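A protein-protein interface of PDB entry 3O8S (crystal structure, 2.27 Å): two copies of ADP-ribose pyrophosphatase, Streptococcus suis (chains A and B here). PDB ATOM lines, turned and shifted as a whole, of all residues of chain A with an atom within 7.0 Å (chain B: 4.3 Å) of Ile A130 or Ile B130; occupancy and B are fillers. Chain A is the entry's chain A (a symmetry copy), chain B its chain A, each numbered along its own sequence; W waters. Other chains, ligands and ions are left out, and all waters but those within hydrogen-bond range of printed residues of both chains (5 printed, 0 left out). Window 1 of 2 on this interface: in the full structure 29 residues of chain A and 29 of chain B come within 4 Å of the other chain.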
ATOM      1  N   LEU A  71      26.945 -14.867  35.404  1.00  0.00           N
ATOM      2  CA  LEU A  71      26.891 -13.893  34.316  1.00  0.00           C
ATOM      3  C   LEU A  71      28.228 -13.195  34.129  1.00  0.00           C
ATOM      4  O   LEU A  71      28.772 -12.650  35.086  1.00  0.00           O
ATOM      5  CB  LEU A  71      25.810 -12.828  34.588  1.00  0.00           C
ATOM      6  CG  LEU A  71      24.528 -12.816  33.739  1.00  0.00           C
ATOM      7  CD1 LEU A  71      23.745 -11.550  33.992  1.00  0.00           C
ATOM      8  CD2 LEU A  71      24.818 -12.888  32.255  1.00  0.00           C
ATOM      9  N   VAL A 106      23.330  -5.379  33.787  1.00  0.00           N
ATOM     10  CA  VAL A 106      24.313  -5.712  32.749  1.00  0.00           C
ATOM     11  C   VAL A 106      25.001  -4.436  32.233  1.00  0.00           C
ATOM     12  O   VAL A 106      26.224  -4.379  32.195  1.00  0.00           O
ATOM     13  CB  VAL A 106      23.645  -6.516  31.593  1.00  0.00           C
ATOM     14  CG1 VAL A 106      24.529  -6.539  30.340  1.00  0.00           C
ATOM     15  CG2 VAL A 106      23.324  -7.931  32.037  1.00  0.00           C
ATOM     16  N   VAL A 127      23.628  -5.282  22.385  1.00  0.00           N
ATOM     17  CA  VAL A 127      23.960  -6.640  22.798  1.00  0.00           C
ATOM     18  C   VAL A 127      24.447  -7.355  21.529  1.00  0.00           C
ATOM     19  O   VAL A 127      23.671  -7.582  20.601  1.00  0.00           O
ATOM     20  CB  VAL A 127      22.810  -7.415  23.509  1.00  0.00           C
ATOM     21  CG1 VAL A 127      23.333  -8.745  24.076  1.00  0.00           C
ATOM     22  CG2 VAL A 127      22.190  -6.573  24.623  1.00  0.00           C
ATOM     23  N   VAL A 128      25.738  -7.657  21.476  1.00  0.00           N
ATOM     24  CA  VAL A 128      26.300  -8.378  20.327  1.00  0.00           C
ATOM     25  C   VAL A 128      25.793  -9.836  20.369  1.00  0.00           C
ATOM     26  O   VAL A 128      25.336 -10.398  19.367  1.00  0.00           O
ATOM     27  CB  VAL A 128      27.867  -8.333  20.310  1.00  0.00           C
ATOM     28  CG1 VAL A 128      28.428  -9.165  19.159  1.00  0.00           C
ATOM     29  CG2 VAL A 128      28.416  -6.899  20.279  1.00  0.00           C
ATOM     30  N   ALA A 129      25.967 -10.447  21.533  1.00  0.00           N
ATOM     31  CA  ALA A 129      25.692 -11.862  21.784  1.00  0.00           C
ATOM     32  C   ALA A 129      25.578 -12.168  23.260  1.00  0.00           C
ATOM     33  O   ALA A 129      26.182 -11.470  24.067  1.00  0.00           O
ATOM     34  CB  ALA A 129      26.815 -12.691  21.193  1.00  0.00           C
ATOM     35  N   ILE A 130      24.774 -13.199  23.601  1.00  0.00           N
ATOM     36  CA  ILE A 130      24.583 -13.822  24.924  1.00  0.00           C
ATOM     37  C   ILE A 130      24.983 -15.267  24.701  1.00  0.00           C
ATOM     38  O   ILE A 130      24.225 -16.021  24.104  1.00  0.00           O
ATOM     39  CB  ILE A 130      23.157 -13.670  25.500  1.00  0.00           C
ATOM     40  CG1 ILE A 130      22.675 -12.238  25.429  1.00  0.00           C
ATOM     41  CG2 ILE A 130      23.038 -14.229  26.913  1.00  0.00           C
ATOM     42  CD1 ILE A 130      21.437 -12.185  24.741  1.00  0.00           C
ATOM     43  N   LEU A 131      26.194 -15.645  25.105  1.00  0.00           N
ATOM     44  CA  LEU A 131      26.689 -16.952  24.746  1.00  0.00           C
ATOM     45  C   LEU A 131      27.074 -17.816  25.908  1.00  0.00           C
ATOM     46  O   LEU A 131      27.641 -17.362  26.886  1.00  0.00           O
ATOM     47  CB  LEU A 131      27.917 -16.784  23.818  1.00  0.00           C
ATOM     48  CG  LEU A 131      27.683 -16.097  22.474  1.00  0.00           C
ATOM     49  CD1 LEU A 131      28.995 -15.647  21.859  1.00  0.00           C
ATOM     50  CD2 LEU A 131      26.866 -16.992  21.518  1.00  0.00           C
ATOM     51  N   ASP A 132      26.828 -19.094  25.748  1.00  0.00           N
ATOM     52  CA  ASP A 132      27.195 -20.086  26.722  1.00  0.00           C
ATOM     53  C   ASP A 132      28.699 -20.361  26.581  1.00  0.00           C
ATOM     54  O   ASP A 132      29.139 -20.796  25.511  1.00  0.00           O
ATOM     55  CB  ASP A 132      26.348 -21.337  26.489  1.00  0.00           C
ATOM     56  CG  ASP A 132      26.680 -22.464  27.415  1.00  0.00           C
ATOM     57  OD1 ASP A 132      26.365 -22.354  28.618  1.00  0.00           O
ATOM     58  OD2 ASP A 132      27.263 -23.450  26.946  1.00  0.00           O
ATOM     59  N   ASN A 136      31.247 -22.008  23.455  1.00  0.00           N
ATOM     60  CA  ASN A 136      32.016 -21.031  22.679  1.00  0.00           C
ATOM     61  C   ASN A 136      33.457 -20.752  23.145  1.00  0.00           C
ATOM     62  O   ASN A 136      34.222 -20.186  22.359  1.00  0.00           O
ATOM     63  CB  ASN A 136      31.253 -19.694  22.677  1.00  0.00           C
ATOM     64  CG  ASN A 136      29.892 -19.789  22.027  1.00  0.00           C
ATOM     65  OD1 ASN A 136      29.747 -19.631  20.808  1.00  0.00           O
ATOM     66  ND2 ASN A 136      28.874 -20.125  22.815  1.00  0.00           N
ATOM     67  N   THR A 146      27.309 -17.705  31.395  1.00  0.00           N
ATOM     68  CA  THR A 146      26.591 -17.076  30.299  1.00  0.00           C
ATOM     69  C   THR A 146      27.365 -15.774  30.060  1.00  0.00           C
ATOM     70  O   THR A 146      27.579 -14.994  31.003  1.00  0.00           O
ATOM     71  CB  THR A 146      25.094 -16.925  30.625  1.00  0.00           C
ATOM     72  OG1 THR A 146      24.458 -18.199  30.474  1.00  0.00           O
ATOM     73  CG2 THR A 146      24.387 -15.901  29.716  1.00  0.00           C
ATOM     74  N   LYS A 147      27.853 -15.578  28.829  1.00  0.00           N
ATOM     75  CA  LYS A 147      28.664 -14.410  28.502  1.00  0.00           C
ATOM     76  C   LYS A 147      27.879 -13.418  27.690  1.00  0.00           C
ATOM     77  O   LYS A 147      27.383 -13.771  26.618  1.00  0.00           O
ATOM     78  CB  LYS A 147      29.921 -14.820  27.728  1.00  0.00           C
ATOM     79  CG  LYS A 147      30.866 -15.731  28.479  1.00  0.00           C
ATOM     80  CD  LYS A 147      31.932 -16.179  27.515  1.00  0.00           C
ATOM     81  CE  LYS A 147      33.318 -15.790  27.932  1.00  0.00           C
ATOM     82  NZ  LYS A 147      33.451 -14.334  28.123  1.00  0.00           N
ATOM     83  N   VAL A 148      27.798 -12.172  28.160  1.00  0.00           N
ATOM     84  CA  VAL A 148      27.089 -11.108  27.422  1.00  0.00           C
ATOM     85  C   VAL A 148      28.140 -10.152  26.829  1.00  0.00           C
ATOM     86  O   VAL A 148      28.887  -9.525  27.574  1.00  0.00           O
ATOM     87  CB  VAL A 148      26.067 -10.352  28.316  1.00  0.00           C
ATOM     88  CG1 VAL A 148      25.245  -9.360  27.498  1.00  0.00           C
ATOM     89  CG2 VAL A 148      25.141 -11.320  29.044  1.00  0.00           C
ATOM     90  N   PHE A 149      28.228 -10.097  25.493  1.00  0.00           N
ATOM     91  CA  PHE A 149      29.110  -9.191  24.767  1.00  0.00           C
ATOM     92  C   PHE A 149      28.311  -7.951  24.446  1.00  0.00           C
ATOM     93  O   PHE A 149      27.275  -8.057  23.803  1.00  0.00           O
ATOM     94  CB  PHE A 149      29.669  -9.856  23.507  1.00  0.00           C
ATOM     95  CG  PHE A 149      30.696 -10.923  23.808  1.00  0.00           C
ATOM     96  CD1 PHE A 149      30.303 -12.225  24.116  1.00  0.00           C
ATOM     97  CD2 PHE A 149      32.059 -10.622  23.810  1.00  0.00           C
ATOM     98  CE1 PHE A 149      31.246 -13.201  24.396  1.00  0.00           C
ATOM     99  CE2 PHE A 149      33.006 -11.604  24.083  1.00  0.00           C
ATOM    100  CZ  PHE A 149      32.592 -12.885  24.374  1.00  0.00           C
ATOM    101  N   ILE A 150      28.759  -6.786  24.939  1.00  0.00           N
ATOM    102  CA  ILE A 150      28.086  -5.512  24.761  1.00  0.00           C
ATOM    103  C   ILE A 150      28.955  -4.585  23.901  1.00  0.00           C
ATOM    104  O   ILE A 150      30.115  -4.333  24.237  1.00  0.00           O
ATOM    105  CB  ILE A 150      27.744  -4.853  26.143  1.00  0.00           C
ATOM    106  CG1 ILE A 150      26.936  -5.820  27.097  1.00  0.00           C
ATOM    107  CG2 ILE A 150      27.079  -3.446  25.991  1.00  0.00           C
ATOM    108  CD1 ILE A 150      25.503  -6.037  26.727  1.00  0.00           C
ATOM    109  N   THR A 203      20.935 -10.014  17.673  1.00  0.00           N
ATOM    110  CA  THR A 203      21.723 -10.479  18.819  1.00  0.00           C
ATOM    111  C   THR A 203      21.823 -12.003  18.787  1.00  0.00           C
ATOM    112  O   THR A 203      20.810 -12.707  18.634  1.00  0.00           O
ATOM    113  CB  THR A 203      21.103  -9.927  20.093  1.00  0.00           C
ATOM    114  OG1 THR A 203      21.264  -8.504  20.067  1.00  0.00           O
ATOM    115  CG2 THR A 203      21.679 -10.552  21.365  1.00  0.00           C
ATOM    116  N   ARG A 204      23.052 -12.505  18.902  1.00  0.00           N
ATOM    117  CA  ARG A 204      23.286 -13.947  18.815  1.00  0.00           C
ATOM    118  C   ARG A 204      23.179 -14.583  20.148  1.00  0.00           C
ATOM    119  O   ARG A 204      23.600 -14.005  21.136  1.00  0.00           O
ATOM    120  CB  ARG A 204      24.660 -14.259  18.196  1.00  0.00           C
ATOM    121  CG  ARG A 204      24.927 -13.528  16.887  1.00  0.00           C
ATOM    122  CD  ARG A 204      23.942 -13.882  15.776  1.00  0.00           C
ATOM    123  NE  ARG A 204      23.826 -12.768  14.841  1.00  0.00           N
ATOM    124  CZ  ARG A 204      24.581 -12.613  13.762  1.00  0.00           C
ATOM    125  NH1 ARG A 204      25.462 -13.538  13.423  1.00  0.00           N
ATOM    126  NH2 ARG A 204      24.449 -11.538  13.005  1.00  0.00           N
ATOM    127  N   PHE A 205      22.666 -15.803  20.191  1.00  0.00           N
ATOM    128  CA  PHE A 205      22.554 -16.508  21.450  1.00  0.00           C
ATOM    129  C   PHE A 205      22.508 -18.000  21.174  1.00  0.00           C
ATOM    130  O   PHE A 205      22.198 -18.396  20.053  1.00  0.00           O
ATOM    131  CB  PHE A 205      21.324 -16.002  22.253  1.00  0.00           C
ATOM    132  CG  PHE A 205      19.955 -16.333  21.696  1.00  0.00           C
ATOM    133  CD1 PHE A 205      19.473 -15.697  20.553  1.00  0.00           C
ATOM    134  CD2 PHE A 205      19.121 -17.230  22.351  1.00  0.00           C
ATOM    135  CE1 PHE A 205      18.197 -15.977  20.053  1.00  0.00           C
ATOM    136  CE2 PHE A 205      17.844 -17.528  21.843  1.00  0.00           C
ATOM    137  CZ  PHE A 205      17.388 -16.893  20.700  1.00  0.00           C
ATOM    138  N   ASP A 206      22.851 -18.828  22.160  1.00  0.00           N
ATOM    139  CA  ASP A 206      22.793 -20.292  21.986  1.00  0.00           C
ATOM    140  C   ASP A 206      22.361 -20.994  23.278  1.00  0.00           C
ATOM    141  O   ASP A 206      21.995 -20.284  24.240  1.00  0.00           O
ATOM    142  CB  ASP A 206      24.137 -20.856  21.479  1.00  0.00           C
ATOM    143  CG  ASP A 206      25.389 -20.508  22.271  1.00  0.00           C
ATOM    144  OD1 ASP A 206      25.263 -20.028  23.422  1.00  0.00           O
ATOM    145  OD2 ASP A 206      26.490 -20.734  21.751  1.00  0.00           O
ATOM    146  OXT ASP A 206      22.311 -22.247  23.301  1.00  0.00           O
ATOM    147  N   VAL B 127      16.403 -12.548  20.834  1.00  0.00           N
ATOM    148  CA  VAL B 127      16.465 -11.953  22.163  1.00  0.00           C
ATOM    149  C   VAL B 127      15.669 -10.643  22.072  1.00  0.00           C
ATOM    150  O   VAL B 127      16.080  -9.708  21.385  1.00  0.00           O
ATOM    151  CB  VAL B 127      17.902 -11.735  22.725  1.00  0.00           C
ATOM    152  CG1 VAL B 127      17.840 -11.299  24.198  1.00  0.00           C
ATOM    153  CG2 VAL B 127      18.742 -13.005  22.583  1.00  0.00           C
ATOM    154  N   ALA B 129      14.769  -8.751  24.808  1.00  0.00           N
ATOM    155  CA  ALA B 129      15.339  -7.907  25.858  1.00  0.00           C
ATOM    156  C   ALA B 129      16.029  -8.718  26.931  1.00  0.00           C
ATOM    157  O   ALA B 129      15.656  -9.866  27.150  1.00  0.00           O
ATOM    158  CB  ALA B 129      14.225  -7.096  26.491  1.00  0.00           C
ATOM    159  N   ILE B 130      17.055  -8.117  27.574  1.00  0.00           N
ATOM    160  CA  ILE B 130      17.810  -8.589  28.748  1.00  0.00           C
ATOM    161  C   ILE B 130      17.593  -7.496  29.777  1.00  0.00           C
ATOM    162  O   ILE B 130      18.191  -6.435  29.670  1.00  0.00           O
ATOM    163  CB  ILE B 130      19.305  -8.874  28.473  1.00  0.00           C
ATOM    164  CG1 ILE B 130      19.493  -9.735  27.245  1.00  0.00           C
ATOM    165  CG2 ILE B 130      20.017  -9.464  29.684  1.00  0.00           C
ATOM    166  CD1 ILE B 130      20.370  -9.090  26.338  1.00  0.00           C
ATOM    167  N   LEU B 131      16.689  -7.714  30.730  1.00  0.00           N
ATOM    168  CA  LEU B 131      16.312  -6.636  31.613  1.00  0.00           C
ATOM    169  C   LEU B 131      16.519  -6.920  33.070  1.00  0.00           C
ATOM    170  O   LEU B 131      16.282  -8.013  33.551  1.00  0.00           O
ATOM    171  CB  LEU B 131      14.820  -6.294  31.376  1.00  0.00           C
ATOM    172  CG  LEU B 131      14.437  -5.783  29.988  1.00  0.00           C
ATOM    173  CD1 LEU B 131      12.937  -5.871  29.774  1.00  0.00           C
ATOM    174  CD2 LEU B 131      14.982  -4.360  29.740  1.00  0.00           C
ATOM    175  N   THR B 146      18.281 -10.902  36.417  1.00  0.00           N
ATOM    176  CA  THR B 146      18.441 -10.451  35.045  1.00  0.00           C
ATOM    177  C   THR B 146      17.436 -11.305  34.263  1.00  0.00           C
ATOM    178  O   THR B 146      17.458 -12.543  34.365  1.00  0.00           O
ATOM    179  CB  THR B 146      19.909 -10.545  34.593  1.00  0.00           C
ATOM    180  OG1 THR B 146      20.641  -9.457  35.168  1.00  0.00           O
ATOM    181  CG2 THR B 146      20.064 -10.501  33.060  1.00  0.00           C
ATOM    182  N   LYS B 147      16.509 -10.650  33.553  1.00  0.00           N
ATOM    183  CA  LYS B 147      15.459 -11.356  32.825  1.00  0.00           C
ATOM    184  C   LYS B 147      15.727 -11.344  31.346  1.00  0.00           C
ATOM    185  O   LYS B 147      15.848 -10.265  30.762  1.00  0.00           O
ATOM    186  CB  LYS B 147      14.091 -10.727  33.100  1.00  0.00           C
ATOM    187  CG  LYS B 147      13.641 -10.779  34.543  1.00  0.00           C
ATOM    188  CD  LYS B 147      12.384  -9.958  34.661  1.00  0.00           C
ATOM    189  CE  LYS B 147      11.201 -10.742  35.143  1.00  0.00           C
ATOM    190  NZ  LYS B 147      10.917 -11.904  34.282  1.00  0.00           N
ATOM    191  N   VAL B 148      15.774 -12.523  30.724  1.00  0.00           N
ATOM    192  CA  VAL B 148      15.986 -12.625  29.267  1.00  0.00           C
ATOM    193  C   VAL B 148      14.654 -13.034  28.614  1.00  0.00           C
ATOM    194  O   VAL B 148      14.139 -14.113  28.897  1.00  0.00           O
ATOM    195  CB  VAL B 148      17.129 -13.615  28.906  1.00  0.00           C
ATOM    196  CG1 VAL B 148      17.428 -13.592  27.410  1.00  0.00           C
ATOM    197  CG2 VAL B 148      18.399 -13.311  29.696  1.00  0.00           C
ATOM    198  N   THR B 203      17.915  -5.526  20.322  1.00  0.00           N
ATOM    199  CA  THR B 203      17.682  -6.139  21.634  1.00  0.00           C
ATOM    200  C   THR B 203      17.822  -5.079  22.726  1.00  0.00           C
ATOM    201  O   THR B 203      18.808  -4.324  22.760  1.00  0.00           O
ATOM    202  CB  THR B 203      18.627  -7.319  21.795  1.00  0.00           C
ATOM    203  OG1 THR B 203      18.242  -8.311  20.835  1.00  0.00           O
ATOM    204  CG2 THR B 203      18.660  -7.877  23.220  1.00  0.00           C
ATOM    205  N   ARG B 204      16.816  -5.010  23.597  1.00  0.00           N
ATOM    206  CA  ARG B 204      16.800  -3.988  24.646  1.00  0.00           C
ATOM    207  C   ARG B 204      17.483  -4.473  25.867  1.00  0.00           C
ATOM    208  O   ARG B 204      17.364  -5.635  26.214  1.00  0.00           O
ATOM    209  CB  ARG B 204      15.363  -3.555  24.989  1.00  0.00           C
ATOM    210  CG  ARG B 204      14.524  -3.181  23.773  1.00  0.00           C
ATOM    211  CD  ARG B 204      15.081  -1.996  22.989  1.00  0.00           C
ATOM    212  NE  ARG B 204      14.671  -2.088  21.591  1.00  0.00           N
ATOM    213  CZ  ARG B 204      13.560  -1.554  21.099  1.00  0.00           C
ATOM    214  NH1 ARG B 204      12.776  -0.817  21.866  1.00  0.00           N
ATOM    215  NH2 ARG B 204      13.235  -1.743  19.833  1.00  0.00           N
ATOM    216  N   PHE B 205      18.165  -3.577  26.566  1.00  0.00           N
ATOM    217  CA  PHE B 205      18.838  -3.960  27.789  1.00  0.00           C
ATOM    218  C   PHE B 205      19.016  -2.728  28.656  1.00  0.00           C
ATOM    219  O   PHE B 205      18.957  -1.614  28.141  1.00  0.00           O
ATOM    220  CB  PHE B 205      20.177  -4.681  27.474  1.00  0.00           C
ATOM    221  CG  PHE B 205      21.285  -3.840  26.871  1.00  0.00           C
ATOM    222  CD1 PHE B 205      21.209  -3.397  25.551  1.00  0.00           C
ATOM    223  CD2 PHE B 205      22.431  -3.549  27.599  1.00  0.00           C
ATOM    224  CE1 PHE B 205      22.244  -2.647  24.979  1.00  0.00           C
ATOM    225  CE2 PHE B 205      23.466  -2.782  27.034  1.00  0.00           C
ATOM    226  CZ  PHE B 205      23.367  -2.342  25.725  1.00  0.00           C
ATOM    227  N   ASP B 206      19.193  -2.905  29.965  1.00  0.00           N
ATOM    228  CA  ASP B 206      19.416  -1.761  30.870  1.00  0.00           C
ATOM    229  C   ASP B 206      20.394  -2.119  31.995  1.00  0.00           C
ATOM    230  O   ASP B 206      20.966  -3.229  31.947  1.00  0.00           O
ATOM    231  CB  ASP B 206      18.089  -1.228  31.448  1.00  0.00           C
ATOM    232  CG  ASP B 206      17.171  -2.227  32.140  1.00  0.00           C
ATOM    233  OD1 ASP B 206      17.630  -3.350  32.457  1.00  0.00           O
ATOM    234  OD2 ASP B 206      16.009  -1.879  32.383  1.00  0.00           O
ATOM    235  OXT ASP B 206      20.648  -1.261  32.874  1.00  0.00           O
HETATM  236  O   HOH W   1      21.000  -4.434  21.308  1.00  0.00           O
HETATM  237  O   HOH W   2      18.287  -8.600  18.135  1.00  0.00           O
HETATM  238  O   HOH W   3      18.288 -11.955  18.625  1.00  0.00           O
HETATM  239  O   HOH W   4      20.689  -6.927  34.067  1.00  0.00           O
HETATM  240  O   HOH W   5      20.288  -6.406  18.644  1.00  0.00           O
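The side-chain hydroxyl (OG1) of Thr B203 sits at hydrogen-bond distance from the side-chain hydroxyl (OG1) of Thr A203 (3.1 Å).
O of Val A127 sits at hydrogen-bond distance from OG1 of Thr A203 (2.6 Å).
The backbone carbonyl oxygen of Val B127 is in hydrogen-bond range of the side-chain hydroxyl of Thr B203 (2.6 Å).
The backbone NH (N) of Ile B130 lies within hydrogen-bond range of the backbone carbonyl oxygen (O) of Arg B204 (2.8 Å).
The backbone NH (N) of Ile A130 lies within hydrogen-bond range of the backbone carbonyl oxygen (O) of Arg A204.
Among the printed residues, pairs that only touch across the chains: Leu A71 with Thr B146, Val A106 with Asp B206, Val A127 with Ile B130, Val A127 with Phe B205, Ile A130 with Val B127, Ile A130 with Ile B130, Ile A150 with Phe B205 and Phe A205 with Val B127.
Of chain B, only Val B127 (3.5 Å) and Ile B130 (3.6 Å) come within 4 Å of Ile A130.
Of chain A, only Val A127 (3.5 Å) and Ile A130 (3.6 Å) come within 4 Å of Ile B130.
Printed residues of chain A within 4 Å of Val B127: Ile A130 (3.5 Å) and Phe A205 (3.4 Å).
Printed residues of chain B within 4 Å of Phe A205: Val B127 (3.4 Å).
Of the printed residues of chain A, Phe B205 touches Val A127 (3.5 Å) and Ile A150 (3.8 Å).
Of the printed residues of chain B, Val A127 touches Ile B130 and Phe B205.
Lys B147 touches none of the printed residues of chain A.
Hydrophobic or aromatic side chains of chain A that line the printed part of chain B: Leu A71, Val A127, Ile A130, Ile A150 and Phe A205.
Hydrophobic or aromatic side chains of chain B that line the printed part of chain A: Val B127, Ile B130 and Phe B205.
Among the printed residues, no Asp or Glu carboxylate lies within 4 Å of a Lys or Arg side-chain nitrogen of the other chain.
Val A127 touches Ile B130, and with the chains exchanged Ile A130 touches Val B127.
Val A127 touches Phe B205, and with the chains exchanged Phe A205 touches Val B127.
Ile B130 touches its own counterpart, Ile A130.
Thr B203 touches its own counterpart, Thr A203.
Positions printed for both chains: 127, 129, 130, 131, 146, 147, 148, 203, 204, 205 and 206.
Of the 9 pairs that touch across the chains among the printed residues, 6 have their exchanged pair printed and touching as well.
Water W3 lies within hydrogen-bond range of O of Thr A203 and N of Val B127.
Water W1 lies within hydrogen-bond range of O of Thr B203 (2.6 Å) and N of Val A127 (3.0 Å).
Water W2 bridges the side-chain hydroxyl (OG1) of Thr B203 (2.7 Å) and the backbone NH (N) of Thr A203 (3.0 Å).
Water W5 bridges the side-chain hydroxyl of Thr A203 (2.7 Å) and the backbone NH of Thr B203 (3.0 Å).
Water W4 bridges OG1 of Thr B146 (2.8 Å) and N of Val A106 (3.1 Å).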
